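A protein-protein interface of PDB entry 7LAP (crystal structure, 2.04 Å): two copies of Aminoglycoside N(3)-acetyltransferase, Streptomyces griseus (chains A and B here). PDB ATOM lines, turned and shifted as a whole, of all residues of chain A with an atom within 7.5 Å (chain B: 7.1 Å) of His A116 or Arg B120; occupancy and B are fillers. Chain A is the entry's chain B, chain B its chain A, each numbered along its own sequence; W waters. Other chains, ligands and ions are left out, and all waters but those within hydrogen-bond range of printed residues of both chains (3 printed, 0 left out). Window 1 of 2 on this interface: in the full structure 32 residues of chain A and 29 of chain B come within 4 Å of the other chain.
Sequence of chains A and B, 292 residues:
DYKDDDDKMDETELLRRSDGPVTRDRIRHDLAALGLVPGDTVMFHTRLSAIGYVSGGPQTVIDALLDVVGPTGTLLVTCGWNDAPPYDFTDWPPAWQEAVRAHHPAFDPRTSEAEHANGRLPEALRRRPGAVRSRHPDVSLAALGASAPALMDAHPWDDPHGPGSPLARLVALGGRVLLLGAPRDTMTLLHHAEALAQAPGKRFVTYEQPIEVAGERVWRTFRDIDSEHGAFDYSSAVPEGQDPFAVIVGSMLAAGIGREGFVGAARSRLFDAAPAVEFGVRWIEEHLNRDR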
ATOM      1  N   CYS A  79      14.290  21.485  20.553  1.00  0.00           N
ATOM      2  CA  CYS A  79      14.668  20.698  19.363  1.00  0.00           C
ATOM      3  C   CYS A  79      16.167  20.706  19.071  1.00  0.00           C
ATOM      4  O   CYS A  79      16.817  19.643  18.995  1.00  0.00           O
ATOM      5  CB  CYS A  79      13.928  21.242  18.116  1.00  0.00           C
ATOM      6  SG  CYS A  79      12.197  20.902  18.121  1.00  0.00           S
ATOM      7  N   GLY A  80      16.755  21.879  18.851  1.00  0.00           N
ATOM      8  CA  GLY A  80      18.121  21.907  18.323  1.00  0.00           C
ATOM      9  C   GLY A  80      18.174  21.329  16.915  1.00  0.00           C
ATOM     10  O   GLY A  80      17.167  21.150  16.250  1.00  0.00           O
ATOM     11  N   TRP A  81      19.391  21.025  16.482  1.00  0.00           N
ATOM     12  CA  TRP A  81      19.667  20.581  15.109  1.00  0.00           C
ATOM     13  C   TRP A  81      20.656  19.420  15.149  1.00  0.00           C
ATOM     14  O   TRP A  81      21.828  19.624  15.486  1.00  0.00           O
ATOM     15  CB  TRP A  81      20.232  21.724  14.277  1.00  0.00           C
ATOM     16  CG  TRP A  81      20.504  21.420  12.846  1.00  0.00           C
ATOM     17  CD1 TRP A  81      20.035  20.340  12.111  1.00  0.00           C
ATOM     18  CD2 TRP A  81      21.336  22.178  11.963  1.00  0.00           C
ATOM     19  NE1 TRP A  81      20.541  20.391  10.836  1.00  0.00           N
ATOM     20  CE2 TRP A  81      21.332  21.514  10.713  1.00  0.00           C
ATOM     21  CE3 TRP A  81      22.056  23.381  12.093  1.00  0.00           C
ATOM     22  CZ2 TRP A  81      22.023  22.013   9.598  1.00  0.00           C
ATOM     23  CZ3 TRP A  81      22.769  23.861  10.985  1.00  0.00           C
ATOM     24  CH2 TRP A  81      22.746  23.178   9.756  1.00  0.00           C
ATOM     25  N   ASN A  82      20.186  18.206  14.812  1.00  0.00           N
ATOM     26  CA  ASN A  82      21.038  17.023  14.937  1.00  0.00           C
ATOM     27  C   ASN A  82      22.238  17.076  14.014  1.00  0.00           C
ATOM     28  O   ASN A  82      23.307  16.569  14.357  1.00  0.00           O
ATOM     29  CB  ASN A  82      20.269  15.737  14.640  1.00  0.00           C
ATOM     30  CG  ASN A  82      20.994  14.520  15.157  1.00  0.00           C
ATOM     31  OD1 ASN A  82      21.054  14.298  16.364  1.00  0.00           O
ATOM     32  ND2 ASN A  82      21.603  13.756  14.257  1.00  0.00           N
ATOM     33  N   ASP A  83      22.083  17.644  12.832  1.00  0.00           N
ATOM     34  CA  ASP A  83      23.131  17.557  11.817  1.00  0.00           C
ATOM     35  C   ASP A  83      23.819  18.898  11.580  1.00  0.00           C
ATOM     36  O   ASP A  83      24.260  19.183  10.467  1.00  0.00           O
ATOM     37  CB  ASP A  83      22.520  17.001  10.539  1.00  0.00           C
ATOM     38  CG  ASP A  83      21.861  15.654  10.803  1.00  0.00           C
ATOM     39  OD1 ASP A  83      22.594  14.771  11.241  1.00  0.00           O
ATOM     40  OD2 ASP A  83      20.626  15.512  10.691  1.00  0.00           O
ATOM     41  N   GLU A 113      16.319  17.915  11.356  1.00  0.00           N
ATOM     42  CA  GLU A 113      15.871  17.099  12.474  1.00  0.00           C
ATOM     43  C   GLU A 113      16.371  17.644  13.787  1.00  0.00           C
ATOM     44  O   GLU A 113      17.465  18.222  13.878  1.00  0.00           O
ATOM     45  CB  GLU A 113      16.319  15.651  12.324  1.00  0.00           C
ATOM     46  CG  GLU A 113      15.894  15.101  11.020  1.00  0.00           C
ATOM     47  CD  GLU A 113      16.699  13.910  10.604  1.00  0.00           C
ATOM     48  OE1 GLU A 113      17.130  13.135  11.499  1.00  0.00           O
ATOM     49  OE2 GLU A 113      16.909  13.777   9.376  1.00  0.00           O
ATOM     50  N   ALA A 114      15.547  17.444  14.811  1.00  0.00           N
ATOM     51  CA  ALA A 114      15.936  17.762  16.169  1.00  0.00           C
ATOM     52  C   ALA A 114      17.102  16.880  16.596  1.00  0.00           C
ATOM     53  O   ALA A 114      17.408  15.868  15.968  1.00  0.00           O
ATOM     54  CB  ALA A 114      14.770  17.569  17.126  1.00  0.00           C
ATOM     55  N   GLU A 115      17.787  17.308  17.655  1.00  0.00           N
ATOM     56  CA  GLU A 115      18.874  16.514  18.204  1.00  0.00           C
ATOM     57  C   GLU A 115      18.344  15.170  18.686  1.00  0.00           C
ATOM     58  O   GLU A 115      17.339  15.110  19.397  1.00  0.00           O
ATOM     59  CB  GLU A 115      19.548  17.264  19.354  1.00  0.00           C
ATOM     60  CG  GLU A 115      20.843  17.971  18.936  1.00  0.00           C
ATOM     61  CD  GLU A 115      21.122  19.248  19.711  1.00  0.00           C
ATOM     62  OE1 GLU A 115      21.049  19.220  20.958  1.00  0.00           O
ATOM     63  OE2 GLU A 115      21.441  20.282  19.083  1.00  0.00           O
ATOM     64  N   HIS A 116      19.054  14.088  18.332  1.00  0.00           N
ATOM     65  CA  HIS A 116      18.593  12.746  18.682  1.00  0.00           C
ATOM     66  C   HIS A 116      18.535  12.534  20.186  1.00  0.00           C
ATOM     67  O   HIS A 116      17.682  11.779  20.678  1.00  0.00           O
ATOM     68  CB  HIS A 116      19.498  11.704  18.049  1.00  0.00           C
ATOM     69  CG  HIS A 116      19.360  11.623  16.565  1.00  0.00           C
ATOM     70  ND1 HIS A 116      18.470  12.410  15.856  1.00  0.00           N
ATOM     71  CD2 HIS A 116      19.994  10.848  15.651  1.00  0.00           C
ATOM     72  CE1 HIS A 116      18.565  12.124  14.571  1.00  0.00           C
ATOM     73  NE2 HIS A 116      19.479  11.176  14.421  1.00  0.00           N
ATOM     74  N   ALA A 117      19.411  13.197  20.933  1.00  0.00           N
ATOM     75  CA  ALA A 117      19.406  13.032  22.381  1.00  0.00           C
ATOM     76  C   ALA A 117      18.103  13.505  23.017  1.00  0.00           C
ATOM     77  O   ALA A 117      17.779  13.070  24.118  1.00  0.00           O
ATOM     78  CB  ALA A 117      20.589  13.778  22.988  1.00  0.00           C
ATOM     79  N   ASN A 118      17.344  14.390  22.367  1.00  0.00           N
ATOM     80  CA  ASN A 118      16.074  14.794  22.964  1.00  0.00           C
ATOM     81  C   ASN A 118      14.970  13.749  22.787  1.00  0.00           C
ATOM     82  O   ASN A 118      13.896  13.894  23.388  1.00  0.00           O
ATOM     83  CB  ASN A 118      15.650  16.150  22.403  1.00  0.00           C
ATOM     84  CG  ASN A 118      16.635  17.247  22.773  1.00  0.00           C
ATOM     85  OD1 ASN A 118      17.384  17.105  23.744  1.00  0.00           O
ATOM     86  ND2 ASN A 118      16.686  18.306  21.977  1.00  0.00           N
ATOM     87  N   GLY A 119      15.226  12.682  22.040  1.00  0.00           N
ATOM     88  CA  GLY A 119      14.287  11.576  21.966  1.00  0.00           C
ATOM     89  C   GLY A 119      13.201  11.869  20.954  1.00  0.00           C
ATOM     90  O   GLY A 119      13.216  12.878  20.253  1.00  0.00           O
ATOM     91  N   ARG A 120      12.256  10.983  20.870  1.00  0.00           N
ATOM     92  CA  ARG A 120      11.215  11.118  19.922  1.00  0.00           C
ATOM     93  C   ARG A 120      10.200  12.210  20.126  1.00  0.00           C
ATOM     94  O   ARG A 120       9.575  12.591  19.193  1.00  0.00           O
ATOM     95  CB  ARG A 120      10.495   9.795  19.757  1.00  0.00           C
ATOM     96  CG  ARG A 120      11.255   8.727  19.028  1.00  0.00           C
ATOM     97  CD  ARG A 120      10.643   7.375  19.324  1.00  0.00           C
ATOM     98  NE  ARG A 120       9.555   7.144  18.425  1.00  0.00           N
ATOM     99  CZ  ARG A 120       8.537   6.340  18.629  1.00  0.00           C
ATOM    100  NH1 ARG A 120       8.442   5.625  19.709  1.00  0.00           N
ATOM    101  NH2 ARG A 120       7.625   6.258  17.708  1.00  0.00           N
ATOM    102  N   PRO A 122      10.229  15.636  20.927  1.00  0.00           N
ATOM    103  CA  PRO A 122      10.388  16.933  20.218  1.00  0.00           C
ATOM    104  C   PRO A 122      10.293  16.789  18.717  1.00  0.00           C
ATOM    105  O   PRO A 122       9.744  17.658  18.042  1.00  0.00           O
ATOM    106  CB  PRO A 122      11.785  17.408  20.655  1.00  0.00           C
ATOM    107  CG  PRO A 122      11.942  16.788  22.046  1.00  0.00           C
ATOM    108  CD  PRO A 122      11.322  15.405  21.888  1.00  0.00           C
ATOM    109  N   GLU A 123      10.800  15.685  18.169  1.00  0.00           N
ATOM    110  CA  GLU A 123      10.708  15.499  16.732  1.00  0.00           C
ATOM    111  C   GLU A 123       9.269  15.206  16.306  1.00  0.00           C
ATOM    112  O   GLU A 123       8.857  15.612  15.217  1.00  0.00           O
ATOM    113  CB  GLU A 123      11.674  14.391  16.299  1.00  0.00           C
ATOM    114  CG  GLU A 123      11.636  14.066  14.847  1.00  0.00           C
ATOM    115  CD  GLU A 123      12.495  15.015  13.971  1.00  0.00           C
ATOM    116  OE1 GLU A 123      12.920  16.100  14.457  1.00  0.00           O
ATOM    117  OE2 GLU A 123      12.688  14.674  12.776  1.00  0.00           O
ATOM    118  N   ARG A 127       6.724  18.135  14.061  1.00  0.00           N
ATOM    119  CA  ARG A 127       6.111  17.715  12.808  1.00  0.00           C
ATOM    120  C   ARG A 127       4.579  17.737  12.867  1.00  0.00           C
ATOM    121  O   ARG A 127       3.930  17.458  11.856  1.00  0.00           O
ATOM    122  CB  ARG A 127       6.646  16.319  12.421  1.00  0.00           C
ATOM    123  CG  ARG A 127       8.217  16.274  12.196  1.00  0.00           C
ATOM    124  CD  ARG A 127       8.818  14.843  12.065  1.00  0.00           C
ATOM    125  NE  ARG A 127       8.275  14.173  10.881  1.00  0.00           N
ATOM    126  CZ  ARG A 127       8.994  13.631   9.893  1.00  0.00           C
ATOM    127  NH1 ARG A 127      10.321  13.663   9.930  1.00  0.00           N
ATOM    128  NH2 ARG A 127       8.369  13.051   8.865  1.00  0.00           N
ATOM    129  N   THR B  46      19.166   2.674   3.142  1.00  0.00           N
ATOM    130  CA  THR B  46      20.346   3.460   3.483  1.00  0.00           C
ATOM    131  C   THR B  46      20.828   3.104   4.874  1.00  0.00           C
ATOM    132  O   THR B  46      20.024   2.996   5.794  1.00  0.00           O
ATOM    133  CB  THR B  46      20.065   4.974   3.459  1.00  0.00           C
ATOM    134  OG1 THR B  46      19.403   5.339   2.250  1.00  0.00           O
ATOM    135  CG2 THR B  46      21.379   5.755   3.548  1.00  0.00           C
ATOM    136  N   LEU B  48      23.270   5.228   6.887  1.00  0.00           N
ATOM    137  CA  LEU B  48      24.076   6.449   6.895  1.00  0.00           C
ATOM    138  C   LEU B  48      25.510   6.299   7.396  1.00  0.00           C
ATOM    139  O   LEU B  48      26.458   6.763   6.762  1.00  0.00           O
ATOM    140  CB  LEU B  48      23.344   7.495   7.721  1.00  0.00           C
ATOM    141  CG  LEU B  48      23.253   8.971   7.415  1.00  0.00           C
ATOM    142  CD1 LEU B  48      23.098   9.215   5.920  1.00  0.00           C
ATOM    143  CD2 LEU B  48      22.021   9.403   8.190  1.00  0.00           C
ATOM    144  N   GLY B  56      25.485  17.332   6.874  1.00  0.00           N
ATOM    145  CA  GLY B  56      24.080  17.597   6.630  1.00  0.00           C
ATOM    146  C   GLY B  56      23.168  16.408   6.837  1.00  0.00           C
ATOM    147  O   GLY B  56      21.956  16.557   6.694  1.00  0.00           O
ATOM    148  N   GLY B  57      23.710  15.225   7.134  1.00  0.00           N
ATOM    149  CA  GLY B  57      22.895  14.056   7.418  1.00  0.00           C
ATOM    150  C   GLY B  57      21.950  13.611   6.308  1.00  0.00           C
ATOM    151  O   GLY B  57      22.257  13.689   5.119  1.00  0.00           O
ATOM    152  N   PRO B  58      20.767  13.112   6.698  1.00  0.00           N
ATOM    153  CA  PRO B  58      19.829  12.559   5.695  1.00  0.00           C
ATOM    154  C   PRO B  58      19.435  13.547   4.610  1.00  0.00           C
ATOM    155  O   PRO B  58      19.213  13.137   3.457  1.00  0.00           O
ATOM    156  CB  PRO B  58      18.600  12.154   6.542  1.00  0.00           C
ATOM    157  CG  PRO B  58      19.147  11.944   7.953  1.00  0.00           C
ATOM    158  CD  PRO B  58      20.281  12.964   8.084  1.00  0.00           C
ATOM    159  N   GLN B  59      19.292  14.833   4.948  1.00  0.00           N
ATOM    160  CA  GLN B  59      18.904  15.831   3.946  1.00  0.00           C
ATOM    161  C   GLN B  59      19.869  15.816   2.774  1.00  0.00           C
ATOM    162  O   GLN B  59      19.465  15.962   1.614  1.00  0.00           O
ATOM    163  CB  GLN B  59      18.864  17.239   4.559  1.00  0.00           C
ATOM    164  CG  GLN B  59      18.359  18.320   3.588  1.00  0.00           C
ATOM    165  CD  GLN B  59      18.568  19.782   4.062  1.00  0.00           C
ATOM    166  OE1 GLN B  59      19.579  20.132   4.652  1.00  0.00           O
ATOM    167  NE2 GLN B  59      17.603  20.622   3.779  1.00  0.00           N
ATOM    168  N   ILE B  62      19.290  12.794   0.422  1.00  0.00           N
ATOM    169  CA  ILE B  62      18.101  12.995  -0.410  1.00  0.00           C
ATOM    170  C   ILE B  62      18.365  14.039  -1.492  1.00  0.00           C
ATOM    171  O   ILE B  62      17.999  13.843  -2.662  1.00  0.00           O
ATOM    172  CB  ILE B  62      16.895  13.376   0.475  1.00  0.00           C
ATOM    173  CG1 ILE B  62      16.523  12.205   1.428  1.00  0.00           C
ATOM    174  CG2 ILE B  62      15.697  13.873  -0.405  1.00  0.00           C
ATOM    175  CD1 ILE B  62      15.561  12.623   2.510  1.00  0.00           C
ATOM    176  N   GLU B 115       8.932   2.902  10.821  1.00  0.00           N
ATOM    177  CA  GLU B 115       9.631   1.964  11.680  1.00  0.00           C
ATOM    178  C   GLU B 115      11.039   2.451  11.961  1.00  0.00           C
ATOM    179  O   GLU B 115      11.780   2.823  11.043  1.00  0.00           O
ATOM    180  CB  GLU B 115       9.665   0.584  11.030  1.00  0.00           C
ATOM    181  CG  GLU B 115       8.290  -0.073  10.998  1.00  0.00           C
ATOM    182  CD  GLU B 115       8.317  -1.480  10.402  1.00  0.00           C
ATOM    183  OE1 GLU B 115       9.421  -2.073  10.369  1.00  0.00           O
ATOM    184  OE2 GLU B 115       7.247  -1.991   9.964  1.00  0.00           O
ATOM    185  N   HIS B 116      11.384   2.470  13.247  1.00  0.00           N
ATOM    186  CA  HIS B 116      12.718   2.866  13.690  1.00  0.00           C
ATOM    187  C   HIS B 116      13.808   2.045  13.009  1.00  0.00           C
ATOM    188  O   HIS B 116      14.896   2.563  12.722  1.00  0.00           O
ATOM    189  CB  HIS B 116      12.844   2.702  15.211  1.00  0.00           C
ATOM    190  CG  HIS B 116      14.254   2.829  15.694  1.00  0.00           C
ATOM    191  ND1 HIS B 116      15.062   1.735  15.934  1.00  0.00           N
ATOM    192  CD2 HIS B 116      15.025   3.923  15.913  1.00  0.00           C
ATOM    193  CE1 HIS B 116      16.262   2.148  16.303  1.00  0.00           C
ATOM    194  NE2 HIS B 116      16.266   3.471  16.298  1.00  0.00           N
ATOM    195  N   ALA B 117      13.527   0.772  12.737  1.00  0.00           N
ATOM    196  CA  ALA B 117      14.511  -0.087  12.107  1.00  0.00           C
ATOM    197  C   ALA B 117      14.795   0.307  10.663  1.00  0.00           C
ATOM    198  O   ALA B 117      15.833  -0.083  10.140  1.00  0.00           O
ATOM    199  CB  ALA B 117      14.046  -1.537  12.152  1.00  0.00           C
ATOM    200  N   ASN B 118      13.893   1.023   9.990  1.00  0.00           N
ATOM    201  CA  ASN B 118      14.193   1.462   8.630  1.00  0.00           C
ATOM    202  C   ASN B 118      15.157   2.653   8.600  1.00  0.00           C
ATOM    203  O   ASN B 118      15.572   3.082   7.514  1.00  0.00           O
ATOM    204  CB  ASN B 118      12.901   1.792   7.881  1.00  0.00           C
ATOM    205  CG  ASN B 118      12.043   0.557   7.638  1.00  0.00           C
ATOM    206  OD1 ASN B 118      12.571  -0.555   7.574  1.00  0.00           O
ATOM    207  ND2 ASN B 118      10.707   0.737   7.555  1.00  0.00           N
ATOM    208  N   GLY B 119      15.561   3.163   9.756  1.00  0.00           N
ATOM    209  CA  GLY B 119      16.559   4.217   9.809  1.00  0.00           C
ATOM    210  C   GLY B 119      15.954   5.591   9.564  1.00  0.00           C
ATOM    211  O   GLY B 119      14.751   5.768   9.386  1.00  0.00           O
ATOM    212  N   ARG B 120      16.832   6.580   9.519  1.00  0.00           N
ATOM    213  CA  ARG B 120      16.401   7.976   9.427  1.00  0.00           C
ATOM    214  C   ARG B 120      16.030   8.434   8.025  1.00  0.00           C
ATOM    215  O   ARG B 120      15.320   9.448   7.904  1.00  0.00           O
ATOM    216  CB  ARG B 120      17.496   8.897   9.966  1.00  0.00           C
ATOM    217  CG  ARG B 120      17.669   8.737  11.475  1.00  0.00           C
ATOM    218  CD  ARG B 120      18.979   9.332  11.896  1.00  0.00           C
ATOM    219  NE  ARG B 120      18.999  10.776  11.662  1.00  0.00           N
ATOM    220  CZ  ARG B 120      20.096  11.495  11.424  1.00  0.00           C
ATOM    221  NH1 ARG B 120      21.290  10.908  11.390  1.00  0.00           N
ATOM    222  NH2 ARG B 120      19.988  12.811  11.244  1.00  0.00           N
ATOM    223  N   LEU B 121      16.500   7.759   6.972  1.00  0.00           N
ATOM    224  CA  LEU B 121      16.181   8.230   5.620  1.00  0.00           C
ATOM    225  C   LEU B 121      14.684   8.197   5.316  1.00  0.00           C
ATOM    226  O   LEU B 121      14.173   9.185   4.760  1.00  0.00           O
ATOM    227  CB  LEU B 121      17.004   7.456   4.580  1.00  0.00           C
ATOM    228  CG  LEU B 121      18.283   8.213   4.158  1.00  0.00           C
ATOM    229  CD1 LEU B 121      17.984   9.550   3.373  1.00  0.00           C
ATOM    230  CD2 LEU B 121      19.181   8.503   5.353  1.00  0.00           C
ATOM    231  N   PRO B 122      13.925   7.134   5.626  1.00  0.00           N
ATOM    232  CA  PRO B 122      12.484   7.170   5.294  1.00  0.00           C
ATOM    233  C   PRO B 122      11.737   8.250   6.041  1.00  0.00           C
ATOM    234  O   PRO B 122      10.821   8.875   5.500  1.00  0.00           O
ATOM    235  CB  PRO B 122      11.998   5.766   5.695  1.00  0.00           C
ATOM    236  CG  PRO B 122      13.270   4.896   5.513  1.00  0.00           C
ATOM    237  CD  PRO B 122      14.384   5.773   5.992  1.00  0.00           C
ATOM    238  N   GLU B 123      12.107   8.477   7.295  1.00  0.00           N
ATOM    239  CA  GLU B 123      11.473   9.513   8.094  1.00  0.00           C
ATOM    240  C   GLU B 123      11.800  10.909   7.549  1.00  0.00           C
ATOM    241  O   GLU B 123      10.948  11.811   7.580  1.00  0.00           O
ATOM    242  CB  GLU B 123      11.908   9.290   9.552  1.00  0.00           C
ATOM    243  CG  GLU B 123      11.107   9.970  10.614  1.00  0.00           C
ATOM    244  CD  GLU B 123       9.619   9.566  10.706  1.00  0.00           C
ATOM    245  OE1 GLU B 123       9.120   8.665   9.993  1.00  0.00           O
ATOM    246  OE2 GLU B 123       8.923  10.247  11.481  1.00  0.00           O
ATOM    247  N   ALA B 124      12.987  11.097   6.971  1.00  0.00           N
ATOM    248  CA  ALA B 124      13.281  12.389   6.364  1.00  0.00           C
ATOM    249  C   ALA B 124      12.585  12.541   5.015  1.00  0.00           C
ATOM    250  O   ALA B 124      12.074  13.621   4.696  1.00  0.00           O
ATOM    251  CB  ALA B 124      14.795  12.568   6.210  1.00  0.00           C
ATOM    252  N   LEU B 125      12.559  11.479   4.211  1.00  0.00           N
ATOM    253  CA  LEU B 125      11.914  11.552   2.901  1.00  0.00           C
ATOM    254  C   LEU B 125      10.443  11.961   3.024  1.00  0.00           C
ATOM    255  O   LEU B 125       9.984  12.892   2.348  1.00  0.00           O
ATOM    256  CB  LEU B 125      12.058  10.197   2.186  1.00  0.00           C
ATOM    257  CG  LEU B 125      11.813   9.975   0.684  1.00  0.00           C
ATOM    258  CD1 LEU B 125      10.355  10.052   0.350  1.00  0.00           C
ATOM    259  CD2 LEU B 125      12.672  10.877  -0.201  1.00  0.00           C
HETATM  260  O   HOH W   1      26.049  16.827   9.366  1.00  0.00           O
HETATM  261  O   HOH W   2      15.001  11.433  10.002  1.00  0.00           O
HETATM  262  O   HOH W   3      20.420  18.903   8.137  1.00  0.00           O
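Of the 18 printed residues of chain B, 6 touch a printed residue of chain A.
Of the 16 printed residues of chain A, 5 touch a printed residue of chain B.
Hydrophobic or aromatic side chains of chain A within 4 Å of the printed part of chain B: His A116.
Among the printed residues, Asp or Glu carboxylates within 4 Å of a Lys or Arg side-chain nitrogen of the other chain: Asp A83 with Arg B120 (2.8 Å), Glu A113 with Arg B120 (2.9 Å) and Arg A127 with Glu B123 (3.9 Å).
His A116 touches Arg B120, but with the chains exchanged Arg A120 does not touch His B116 (6.4 Å).
Positions printed for both chains: 115, 116, 117, 118, 119, 120, 122 and 123.
Of the 10 pairs that touch across the chains among the printed residues, none has its exchanged pair printed and touching as well.
The side-chain amide nitrogen of Asn A82 is in hydrogen-bond range of the side-chain carboxylate of Asp A83 (3.3 Å).
OE2 of Glu A123 is in salt-bridge range of NH1 of Arg A127 (3.8 Å).
N of Asn A82 is in hydrogen-bond range of O of Glu A113, at 2.9 Å.
OD1 of Asn A82 is in hydrogen-bond range of N of His A116 (2.8 Å).
Printed residues of chain B within 4 Å of Arg A127: Glu B123 (3.1 Å).
Printed residues of chain A within 4 Å of Gly B56: Asp A83 (3.8 Å).
Of the printed residues of chain A, Gly B57 touches Asp A83 (3.9 Å).
His B116 touches none of the printed residues of chain A.
Arg B120 touches four residues of chain A.
The nearest residue of chain A that does not touch Arg B120 is Ala A114 (6.2 Å).
Water W1 bridges the backbone NH of Gly B56 and the backbone carbonyl oxygen of Asp A83.
Water W2 bridges the backbone carbonyl oxygen (O) of Arg B120 (2.9 Å) and the side-chain carboxylate (OE2) of Glu A113 (3.1 Å).
Water W3 lies within hydrogen-bond range of NE1 of Trp A81 and O of Gly B56.
NH2 of Arg A127 lies within salt-bridge range of OE2 of Glu B123.
The guanidinium group (NH2) of Arg B120 is in salt-bridge range of the side-chain carboxylate (OE1) of Glu A113, 2.9 Å away.
The guanidinium group of Arg B120 lies within salt-bridge range of the side-chain carboxylate of Asp A83 (2.8 Å).
NE of Arg B120 sits at hydrogen-bond distance from NE2 of His A116.
Among the printed residues, pairs that only touch across the chains: Glu A113 with Pro B58 (3.2 Å), Asn A82 with Arg B120 (3.5 Å), Asp A83 with Pro B58 (3.7 Å), Asp A83 with Gly B56 (3.8 Å), Asp A83 with Gly B57 (3.9 Å) and Glu A113 with Ala B124 (3.99 Å).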
